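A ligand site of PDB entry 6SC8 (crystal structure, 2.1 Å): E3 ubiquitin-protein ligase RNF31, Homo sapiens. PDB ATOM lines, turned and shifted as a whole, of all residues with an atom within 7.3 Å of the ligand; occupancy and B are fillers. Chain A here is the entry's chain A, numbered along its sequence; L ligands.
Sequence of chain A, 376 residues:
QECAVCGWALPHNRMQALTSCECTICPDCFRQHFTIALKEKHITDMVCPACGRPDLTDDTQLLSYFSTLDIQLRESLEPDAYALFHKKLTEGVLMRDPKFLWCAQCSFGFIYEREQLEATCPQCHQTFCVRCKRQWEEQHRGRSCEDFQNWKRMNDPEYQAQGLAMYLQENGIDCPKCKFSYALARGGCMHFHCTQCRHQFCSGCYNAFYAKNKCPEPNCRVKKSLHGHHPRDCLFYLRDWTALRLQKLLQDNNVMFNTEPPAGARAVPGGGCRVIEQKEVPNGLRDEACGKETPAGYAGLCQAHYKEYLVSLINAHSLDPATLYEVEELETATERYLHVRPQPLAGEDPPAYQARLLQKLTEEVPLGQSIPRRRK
A ring nitrogen (NE2) of His 191 lies within hydrogen-bond range of a ring nitrogen (NE2) of His 193, 3.4 Å away.
The backbone NH (N) of Phe 192 sits at hydrogen-bond distance from the backbone carbonyl oxygen (O) of Phe 201 (2.8 Å).
The backbone NH (N) of Thr 195 lies within hydrogen-bond range of the side-chain hydroxyl (OH) of Tyr 182.
OE1 of Gln 196 lies within hydrogen-bond range of OG1 of Thr 195, 2.5 Å away.
OH of Tyr 182 lies close to SG of Cys 194 (2.7 Å).
The backbone carbonyl oxygen (O) of Ile 173 lies within hydrogen-bond range of the backbone NH (N) of Tyr 182 (2.9 Å).
OH of Tyr 182 sits at hydrogen-bond distance from OE1 of Gln 196, at 2.6 Å.
Tyr 182 touches the ligand (CD2 to C6, 3.9 Å).
Leu 184 touches the ligand.
Phe 192 touches the ligand.
Thr 195 touches the ligand.
Hydrophobic or aromatic side chains that line the ligand: Tyr 182, Leu 184, Phe 192 and His 193.
Seven residues have an atom within 4 Å of the ligand: Tyr 182, Leu 184, Cys 189, His 191, Phe 192, His 193 and Thr 195.
The side-chain sulfur (SG) of Cys 189 is covalently linked to a carbon (C14) of the ligand (1.8 Å).
N of His 193 is in hydrogen-bond range of O2 of the ligand (2.7 Å).
The backbone carbonyl oxygen (O) of His 193 sits at hydrogen-bond distance from a nitrogen (N2) of the ligand (2.7 Å).
The backbone carbonyl oxygen (O) of His 191 lies close to a nitrogen (N1) of the ligand (3.3 Å).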
ATOM      1  N   ILE A 173      32.033   0.364 -16.006  1.00  0.00           N
ATOM      2  CA  ILE A 173      30.878  -0.491 -15.747  1.00  0.00           C
ATOM      3  C   ILE A 173      30.287  -0.847 -17.096  1.00  0.00           C
ATOM      4  O   ILE A 173      29.772   0.022 -17.815  1.00  0.00           O
ATOM      5  CB  ILE A 173      29.846   0.215 -14.845  1.00  0.00           C
ATOM      6  CG1 ILE A 173      30.491   0.624 -13.518  1.00  0.00           C
ATOM      7  CG2 ILE A 173      28.628  -0.686 -14.616  1.00  0.00           C
ATOM      8  CD1 ILE A 173      29.554   1.356 -12.586  1.00  0.00           C
ATOM      9  N   PHE A 180      27.202  -1.543 -23.369  1.00  0.00           N
ATOM     10  CA  PHE A 180      27.609  -0.154 -23.206  1.00  0.00           C
ATOM     11  C   PHE A 180      28.498  -0.020 -21.977  1.00  0.00           C
ATOM     12  O   PHE A 180      28.166  -0.520 -20.896  1.00  0.00           O
ATOM     13  CB  PHE A 180      26.394   0.761 -23.085  1.00  0.00           C
ATOM     14  CG  PHE A 180      26.724   2.231 -23.072  1.00  0.00           C
ATOM     15  CD1 PHE A 180      27.245   2.842 -21.936  1.00  0.00           C
ATOM     16  CD2 PHE A 180      26.495   3.018 -24.189  1.00  0.00           C
ATOM     17  CE1 PHE A 180      27.546   4.184 -21.916  1.00  0.00           C
ATOM     18  CE2 PHE A 180      26.793   4.380 -24.178  1.00  0.00           C
ATOM     19  CZ  PHE A 180      27.322   4.957 -23.032  1.00  0.00           C
ATOM     20  N   TYR A 182      30.131   2.469 -19.256  1.00  0.00           N
ATOM     21  CA  TYR A 182      29.775   3.766 -18.704  1.00  0.00           C
ATOM     22  C   TYR A 182      30.953   4.519 -18.100  1.00  0.00           C
ATOM     23  O   TYR A 182      30.933   5.753 -18.064  1.00  0.00           O
ATOM     24  CB  TYR A 182      28.676   3.602 -17.647  1.00  0.00           C
ATOM     25  CG  TYR A 182      27.326   3.338 -18.250  1.00  0.00           C
ATOM     26  CD1 TYR A 182      26.947   2.057 -18.616  1.00  0.00           C
ATOM     27  CD2 TYR A 182      26.426   4.379 -18.480  1.00  0.00           C
ATOM     28  CE1 TYR A 182      25.704   1.801 -19.176  1.00  0.00           C
ATOM     29  CE2 TYR A 182      25.186   4.139 -19.037  1.00  0.00           C
ATOM     30  CZ  TYR A 182      24.828   2.851 -19.391  1.00  0.00           C
ATOM     31  OH  TYR A 182      23.596   2.615 -19.943  1.00  0.00           O
ATOM     32  N   LEU A 184      32.225   4.836 -14.864  1.00  0.00           N
ATOM     33  CA  LEU A 184      31.885   5.575 -13.667  1.00  0.00           C
ATOM     34  C   LEU A 184      32.355   4.799 -12.448  1.00  0.00           C
ATOM     35  O   LEU A 184      32.555   3.591 -12.497  1.00  0.00           O
ATOM     36  CB  LEU A 184      30.382   5.832 -13.546  1.00  0.00           C
ATOM     37  CG  LEU A 184      29.611   6.395 -14.736  1.00  0.00           C
ATOM     38  CD1 LEU A 184      28.252   5.741 -14.801  1.00  0.00           C
ATOM     39  CD2 LEU A 184      29.490   7.903 -14.621  1.00  0.00           C
ATOM     40  N   ALA A 185      32.529   5.520 -11.349  1.00  0.00           N
ATOM     41  CA  ALA A 185      32.738   4.861 -10.071  1.00  0.00           C
ATOM     42  C   ALA A 185      31.417   4.274  -9.575  1.00  0.00           C
ATOM     43  O   ALA A 185      30.339   4.600 -10.063  1.00  0.00           O
ATOM     44  CB  ALA A 185      33.311   5.822  -9.040  1.00  0.00           C
ATOM     45  N   ARG A 186      31.528   3.385  -8.587  1.00  0.00           N
ATOM     46  CA  ARG A 186      30.354   2.725  -8.023  1.00  0.00           C
ATOM     47  C   ARG A 186      29.887   3.358  -6.726  1.00  0.00           C
ATOM     48  O   ARG A 186      28.679   3.488  -6.508  1.00  0.00           O
ATOM     49  CB  ARG A 186      30.660   1.243  -7.784  1.00  0.00           C
ATOM     50  CG  ARG A 186      30.177   0.349  -8.888  1.00  0.00           C
ATOM     51  CD  ARG A 186      31.321  -0.167  -9.730  1.00  0.00           C
ATOM     52  NE  ARG A 186      32.168  -1.085  -8.986  1.00  0.00           N
ATOM     53  CZ  ARG A 186      32.920  -2.017  -9.534  1.00  0.00           C
ATOM     54  NH1 ARG A 186      33.665  -2.817  -8.773  1.00  0.00           N
ATOM     55  NH2 ARG A 186      32.947  -2.159 -10.850  1.00  0.00           N
ATOM     56  N   GLY A 187      30.813   3.773  -5.867  1.00  0.00           N
ATOM     57  CA  GLY A 187      30.401   4.304  -4.580  1.00  0.00           C
ATOM     58  C   GLY A 187      29.783   3.214  -3.735  1.00  0.00           C
ATOM     59  O   GLY A 187      30.333   2.102  -3.631  1.00  0.00           O
ATOM     60  N   GLY A 188      28.641   3.507  -3.128  1.00  0.00           N
ATOM     61  CA  GLY A 188      27.986   2.564  -2.251  1.00  0.00           C
ATOM     62  C   GLY A 188      26.746   1.920  -2.840  1.00  0.00           C
ATOM     63  O   GLY A 188      26.172   1.014  -2.232  1.00  0.00           O
ATOM     64  N   CYS A 189      26.336   2.375  -4.018  1.00  0.00           N
ATOM     65  CA  CYS A 189      25.121   1.889  -4.669  1.00  0.00           C
ATOM     66  C   CYS A 189      25.484   0.831  -5.701  1.00  0.00           C
ATOM     67  O   CYS A 189      26.159   1.127  -6.698  1.00  0.00           O
ATOM     68  CB  CYS A 189      24.353   3.035  -5.320  1.00  0.00           C
ATOM     69  SG  CYS A 189      22.719   2.545  -5.936  1.00  0.00           S
ATOM     70  N   MET A 190      25.010  -0.402  -5.492  1.00  0.00           N
ATOM     71  CA  MET A 190      25.298  -1.496  -6.414  1.00  0.00           C
ATOM     72  C   MET A 190      24.235  -1.662  -7.491  1.00  0.00           C
ATOM     73  O   MET A 190      24.557  -2.158  -8.582  1.00  0.00           O
ATOM     74  CB  MET A 190      25.424  -2.811  -5.637  1.00  0.00           C
ATOM     75  CG  MET A 190      26.308  -2.731  -4.407  1.00  0.00           C
ATOM     76  SD  MET A 190      27.970  -2.167  -4.806  1.00  0.00           S
ATOM     77  CE  MET A 190      28.476  -3.430  -5.952  1.00  0.00           C
ATOM     78  N   HIS A 191      22.995  -1.277  -7.214  1.00  0.00           N
ATOM     79  CA  HIS A 191      21.894  -1.480  -8.161  1.00  0.00           C
ATOM     80  C   HIS A 191      22.033  -0.505  -9.320  1.00  0.00           C
ATOM     81  O   HIS A 191      21.762   0.688  -9.182  1.00  0.00           O
ATOM     82  CB  HIS A 191      20.557  -1.305  -7.436  1.00  0.00           C
ATOM     83  CG  HIS A 191      19.374  -1.708  -8.257  1.00  0.00           C
ATOM     84  ND1 HIS A 191      18.111  -1.833  -7.718  1.00  0.00           N
ATOM     85  CD2 HIS A 191      19.256  -2.008  -9.576  1.00  0.00           C
ATOM     86  CE1 HIS A 191      17.265  -2.194  -8.666  1.00  0.00           C
ATOM     87  NE2 HIS A 191      17.933  -2.309  -9.804  1.00  0.00           N
ATOM     88  N   PHE A 192      22.427  -1.015 -10.486  1.00  0.00           N
ATOM     89  CA  PHE A 192      22.660  -0.192 -11.669  1.00  0.00           C
ATOM     90  C   PHE A 192      21.486  -0.301 -12.633  1.00  0.00           C
ATOM     91  O   PHE A 192      20.923  -1.386 -12.826  1.00  0.00           O
ATOM     92  CB  PHE A 192      23.946  -0.597 -12.367  1.00  0.00           C
ATOM     93  CG  PHE A 192      24.541   0.486 -13.209  1.00  0.00           C
ATOM     94  CD1 PHE A 192      25.409   1.418 -12.666  1.00  0.00           C
ATOM     95  CD2 PHE A 192      24.221   0.581 -14.560  1.00  0.00           C
ATOM     96  CE1 PHE A 192      25.959   2.418 -13.442  1.00  0.00           C
ATOM     97  CE2 PHE A 192      24.759   1.592 -15.343  1.00  0.00           C
ATOM     98  CZ  PHE A 192      25.624   2.509 -14.786  1.00  0.00           C
ATOM     99  N   HIS A 193      21.138   0.826 -13.239  1.00  0.00           N
ATOM    100  CA  HIS A 193      20.124   0.894 -14.279  1.00  0.00           C
ATOM    101  C   HIS A 193      20.779   1.395 -15.562  1.00  0.00           C
ATOM    102  O   HIS A 193      21.420   2.447 -15.564  1.00  0.00           O
ATOM    103  CB  HIS A 193      18.973   1.834 -13.886  1.00  0.00           C
ATOM    104  CG  HIS A 193      18.311   1.459 -12.588  1.00  0.00           C
ATOM    105  ND1 HIS A 193      18.859   1.753 -11.357  1.00  0.00           N
ATOM    106  CD2 HIS A 193      17.139   0.821 -12.337  1.00  0.00           C
ATOM    107  CE1 HIS A 193      18.060   1.309 -10.407  1.00  0.00           C
ATOM    108  NE2 HIS A 193      17.013   0.742 -10.980  1.00  0.00           N
ATOM    109  N   CYS A 194      20.626   0.636 -16.653  1.00  0.00           N
ATOM    110  CA  CYS A 194      21.220   1.022 -17.922  1.00  0.00           C
ATOM    111  C   CYS A 194      20.218   1.823 -18.744  1.00  0.00           C
ATOM    112  O   CYS A 194      19.064   1.419 -18.903  1.00  0.00           O
ATOM    113  CB  CYS A 194      21.695  -0.207 -18.703  1.00  0.00           C
ATOM    114  SG  CYS A 194      22.421   0.171 -20.321  1.00  0.00           S
ATOM    115  N   THR A 195      20.676   2.961 -19.261  1.00  0.00           N
ATOM    116  CA  THR A 195      19.787   3.851 -19.998  1.00  0.00           C
ATOM    117  C   THR A 195      19.372   3.246 -21.342  1.00  0.00           C
ATOM    118  O   THR A 195      18.234   3.424 -21.778  1.00  0.00           O
ATOM    119  CB  THR A 195      20.458   5.214 -20.210  1.00  0.00           C
ATOM    120  OG1 THR A 195      21.623   5.036 -21.014  1.00  0.00           O
ATOM    121  CG2 THR A 195      20.874   5.796 -18.875  1.00  0.00           C
ATOM    122  N   GLN A 196      20.280   2.510 -21.992  1.00  0.00           N
ATOM    123  CA  GLN A 196      19.987   2.026 -23.332  1.00  0.00           C
ATOM    124  C   GLN A 196      19.046   0.833 -23.329  1.00  0.00           C
ATOM    125  O   GLN A 196      18.100   0.791 -24.121  1.00  0.00           O
ATOM    126  CB  GLN A 196      21.288   1.660 -24.059  1.00  0.00           C
ATOM    127  CG  GLN A 196      22.054   2.850 -24.596  1.00  0.00           C
ATOM    128  CD  GLN A 196      22.571   3.733 -23.482  1.00  0.00           C
ATOM    129  OE1 GLN A 196      22.816   3.271 -22.371  1.00  0.00           O
ATOM    130  NE2 GLN A 196      22.735   5.023 -23.777  1.00  0.00           N
ATOM    131  N   HIS A 199      18.271  -2.670 -18.525  1.00  0.00           N
ATOM    132  CA  HIS A 199      18.676  -3.796 -17.701  1.00  0.00           C
ATOM    133  C   HIS A 199      19.088  -3.307 -16.319  1.00  0.00           C
ATOM    134  O   HIS A 199      19.759  -2.282 -16.168  1.00  0.00           O
ATOM    135  CB  HIS A 199      19.835  -4.542 -18.358  1.00  0.00           C
ATOM    136  CG  HIS A 199      20.178  -5.834 -17.678  1.00  0.00           C
ATOM    137  ND1 HIS A 199      19.230  -6.783 -17.360  1.00  0.00           N
ATOM    138  CD2 HIS A 199      21.362  -6.343 -17.275  1.00  0.00           C
ATOM    139  CE1 HIS A 199      19.816  -7.822 -16.778  1.00  0.00           C
ATOM    140  NE2 HIS A 199      21.110  -7.576 -16.717  1.00  0.00           N
ATOM    141  N   PHE A 201      21.173  -4.498 -13.011  1.00  0.00           N
ATOM    142  CA  PHE A 201      22.202  -5.454 -12.639  1.00  0.00           C
ATOM    143  C   PHE A 201      23.061  -4.850 -11.535  1.00  0.00           C
ATOM    144  O   PHE A 201      23.037  -3.649 -11.285  1.00  0.00           O
ATOM    145  CB  PHE A 201      23.073  -5.839 -13.848  1.00  0.00           C
ATOM    146  CG  PHE A 201      23.878  -4.698 -14.400  1.00  0.00           C
ATOM    147  CD1 PHE A 201      23.302  -3.798 -15.286  1.00  0.00           C
ATOM    148  CD2 PHE A 201      25.208  -4.524 -14.040  1.00  0.00           C
ATOM    149  CE1 PHE A 201      24.047  -2.740 -15.805  1.00  0.00           C
ATOM    150  CE2 PHE A 201      25.946  -3.468 -14.547  1.00  0.00           C
ATOM    151  CZ  PHE A 201      25.367  -2.583 -15.437  1.00  0.00           C
ATOM    152  N   SER A 203      26.532  -3.649 -10.207  1.00  0.00           N
ATOM    153  CA  SER A 203      27.764  -3.143 -10.791  1.00  0.00           C
ATOM    154  C   SER A 203      29.013  -3.817 -10.227  1.00  0.00           C
ATOM    155  O   SER A 203      30.103  -3.652 -10.787  1.00  0.00           O
ATOM    156  CB  SER A 203      27.860  -1.626 -10.596  1.00  0.00           C
ATOM    157  OG  SER A 203      27.548  -1.274  -9.259  1.00  0.00           O
ATOM    158  N   GLU A 277      30.507  11.976  -9.996  1.00  0.00           N
ATOM    159  CA  GLU A 277      29.261  11.232 -10.134  1.00  0.00           C
ATOM    160  C   GLU A 277      28.378  11.933 -11.157  1.00  0.00           C
ATOM    161  O   GLU A 277      28.501  13.132 -11.409  1.00  0.00           O
ATOM    162  CB  GLU A 277      28.529  11.115  -8.798  1.00  0.00           C
ATOM    163  CG  GLU A 277      29.387  10.626  -7.659  1.00  0.00           C
ATOM    164  CD  GLU A 277      28.574  10.242  -6.429  1.00  0.00           C
ATOM    165  OE1 GLU A 277      29.044   9.411  -5.636  1.00  0.00           O
ATOM    166  OE2 GLU A 277      27.456  10.781  -6.275  1.00  0.00           O
ATOM    167  N   GLN A 278      27.459  11.167 -11.740  1.00  0.00           N
ATOM    168  CA  GLN A 278      26.560  11.674 -12.779  1.00  0.00           C
ATOM    169  C   GLN A 278      25.174  11.883 -12.160  1.00  0.00           C
ATOM    170  O   GLN A 278      24.350  10.970 -12.119  1.00  0.00           O
ATOM    171  CB  GLN A 278      26.511  10.724 -13.965  1.00  0.00           C
ATOM    172  CG  GLN A 278      27.545  11.022 -15.039  1.00  0.00           C
ATOM    173  CD  GLN A 278      27.083  12.091 -16.020  1.00  0.00           C
ATOM    174  N   LYS A 279      24.934  13.099 -11.671  1.00  0.00           N
ATOM    175  CA  LYS A 279      23.647  13.467 -11.114  1.00  0.00           C
ATOM    176  C   LYS A 279      22.713  13.965 -12.214  1.00  0.00           C
ATOM    177  O   LYS A 279      23.137  14.697 -13.121  1.00  0.00           O
ATOM    178  CB  LYS A 279      23.814  14.548 -10.048  1.00  0.00           C
ATOM    179  N   GLU A 280      21.446  13.579 -12.126  1.00  0.00           N
ATOM    180  CA  GLU A 280      20.473  13.892 -13.164  1.00  0.00           C
ATOM    181  C   GLU A 280      19.833  15.244 -12.870  1.00  0.00           C
ATOM    182  O   GLU A 280      19.289  15.468 -11.785  1.00  0.00           O
ATOM    183  CB  GLU A 280      19.397  12.797 -13.244  1.00  0.00           C
ATOM    184  CG  GLU A 280      18.615  12.801 -14.557  1.00  0.00           C
ATOM    185  CD  GLU A 280      18.633  11.458 -15.251  1.00  0.00           C
ATOM    186  OE1 GLU A 280      18.544  11.427 -16.500  1.00  0.00           O
ATOM    187  OE2 GLU A 280      18.724  10.422 -14.553  1.00  0.00           O
ATOM    188  N   LEU A 285      22.614  15.078 -17.678  1.00  0.00           N
ATOM    189  CA  LEU A 285      23.339  14.603 -16.506  1.00  0.00           C
ATOM    190  C   LEU A 285      24.426  15.622 -16.167  1.00  0.00           C
ATOM    191  O   LEU A 285      25.245  15.976 -17.031  1.00  0.00           O
ATOM    192  CB  LEU A 285      23.963  13.234 -16.762  1.00  0.00           C
ATOM    193  CG  LEU A 285      23.044  12.012 -16.903  1.00  0.00           C
ATOM    194  CD1 LEU A 285      23.851  10.732 -16.840  1.00  0.00           C
ATOM    195  CD2 LEU A 285      21.958  12.031 -15.841  1.00  0.00           C
HETATM  196  C1  LIG L   1      24.488   5.649 -12.424  1.00  0.00           C
HETATM  197  N1  LIG L   1      23.349   3.509  -9.650  1.00  0.00           N
HETATM  198  C2  LIG L   1      23.694   3.110  -8.292  1.00  0.00           C
HETATM  199  C3  LIG L   1      22.683   5.255  -7.452  1.00  0.00           C
HETATM  200  C4  LIG L   1      23.407   8.242  -2.167  1.00  0.00           C
HETATM  201  C5  LIG L   1      24.921   7.041 -14.465  1.00  0.00           C
HETATM  202  C6  LIG L   1      24.788   6.882 -15.975  1.00  0.00           C
HETATM  203  C7  LIG L   1      23.330   6.724 -16.355  1.00  0.00           C
HETATM  204  C8  LIG L   1      22.790   5.369 -15.892  1.00  0.00           C
HETATM  205  C9  LIG L   1      23.151   5.110 -14.442  1.00  0.00           C
HETATM  206  C10 LIG L   1      24.186   5.916 -13.752  1.00  0.00           C
HETATM  207  C11 LIG L   1      22.797   3.837 -12.511  1.00  0.00           C
HETATM  208  C12 LIG L   1      23.823   4.623 -11.770  1.00  0.00           C
HETATM  209  C13 LIG L   1      24.147   4.305 -10.345  1.00  0.00           C
HETATM  210  C14 LIG L   1      22.776   3.740  -7.244  1.00  0.00           C
HETATM  211  C15 LIG L   1      22.148   5.956  -6.228  1.00  0.00           C
HETATM  212  C16 LIG L   1      22.659   8.000  -4.889  1.00  0.00           C
HETATM  213  C17 LIG L   1      24.013   7.522  -4.422  1.00  0.00           C
HETATM  214  N2  LIG L   1      22.524   4.125 -13.796  1.00  0.00           N
HETATM  215  N3  LIG L   1      24.235   7.512  -3.102  1.00  0.00           N
HETATM  216  O1  LIG L   1      22.324   7.401  -6.124  1.00  0.00           O
HETATM  217  O2  LIG L   1      22.194   2.911 -11.944  1.00  0.00           O
HETATM  218  O3  LIG L   1      25.151   4.798  -9.858  1.00  0.00           O
HETATM  219  O4  LIG L   1      21.544   5.366  -5.353  1.00  0.00           O
HETATM  220  O5  LIG L   1      24.852   7.158  -5.234  1.00  0.00           O
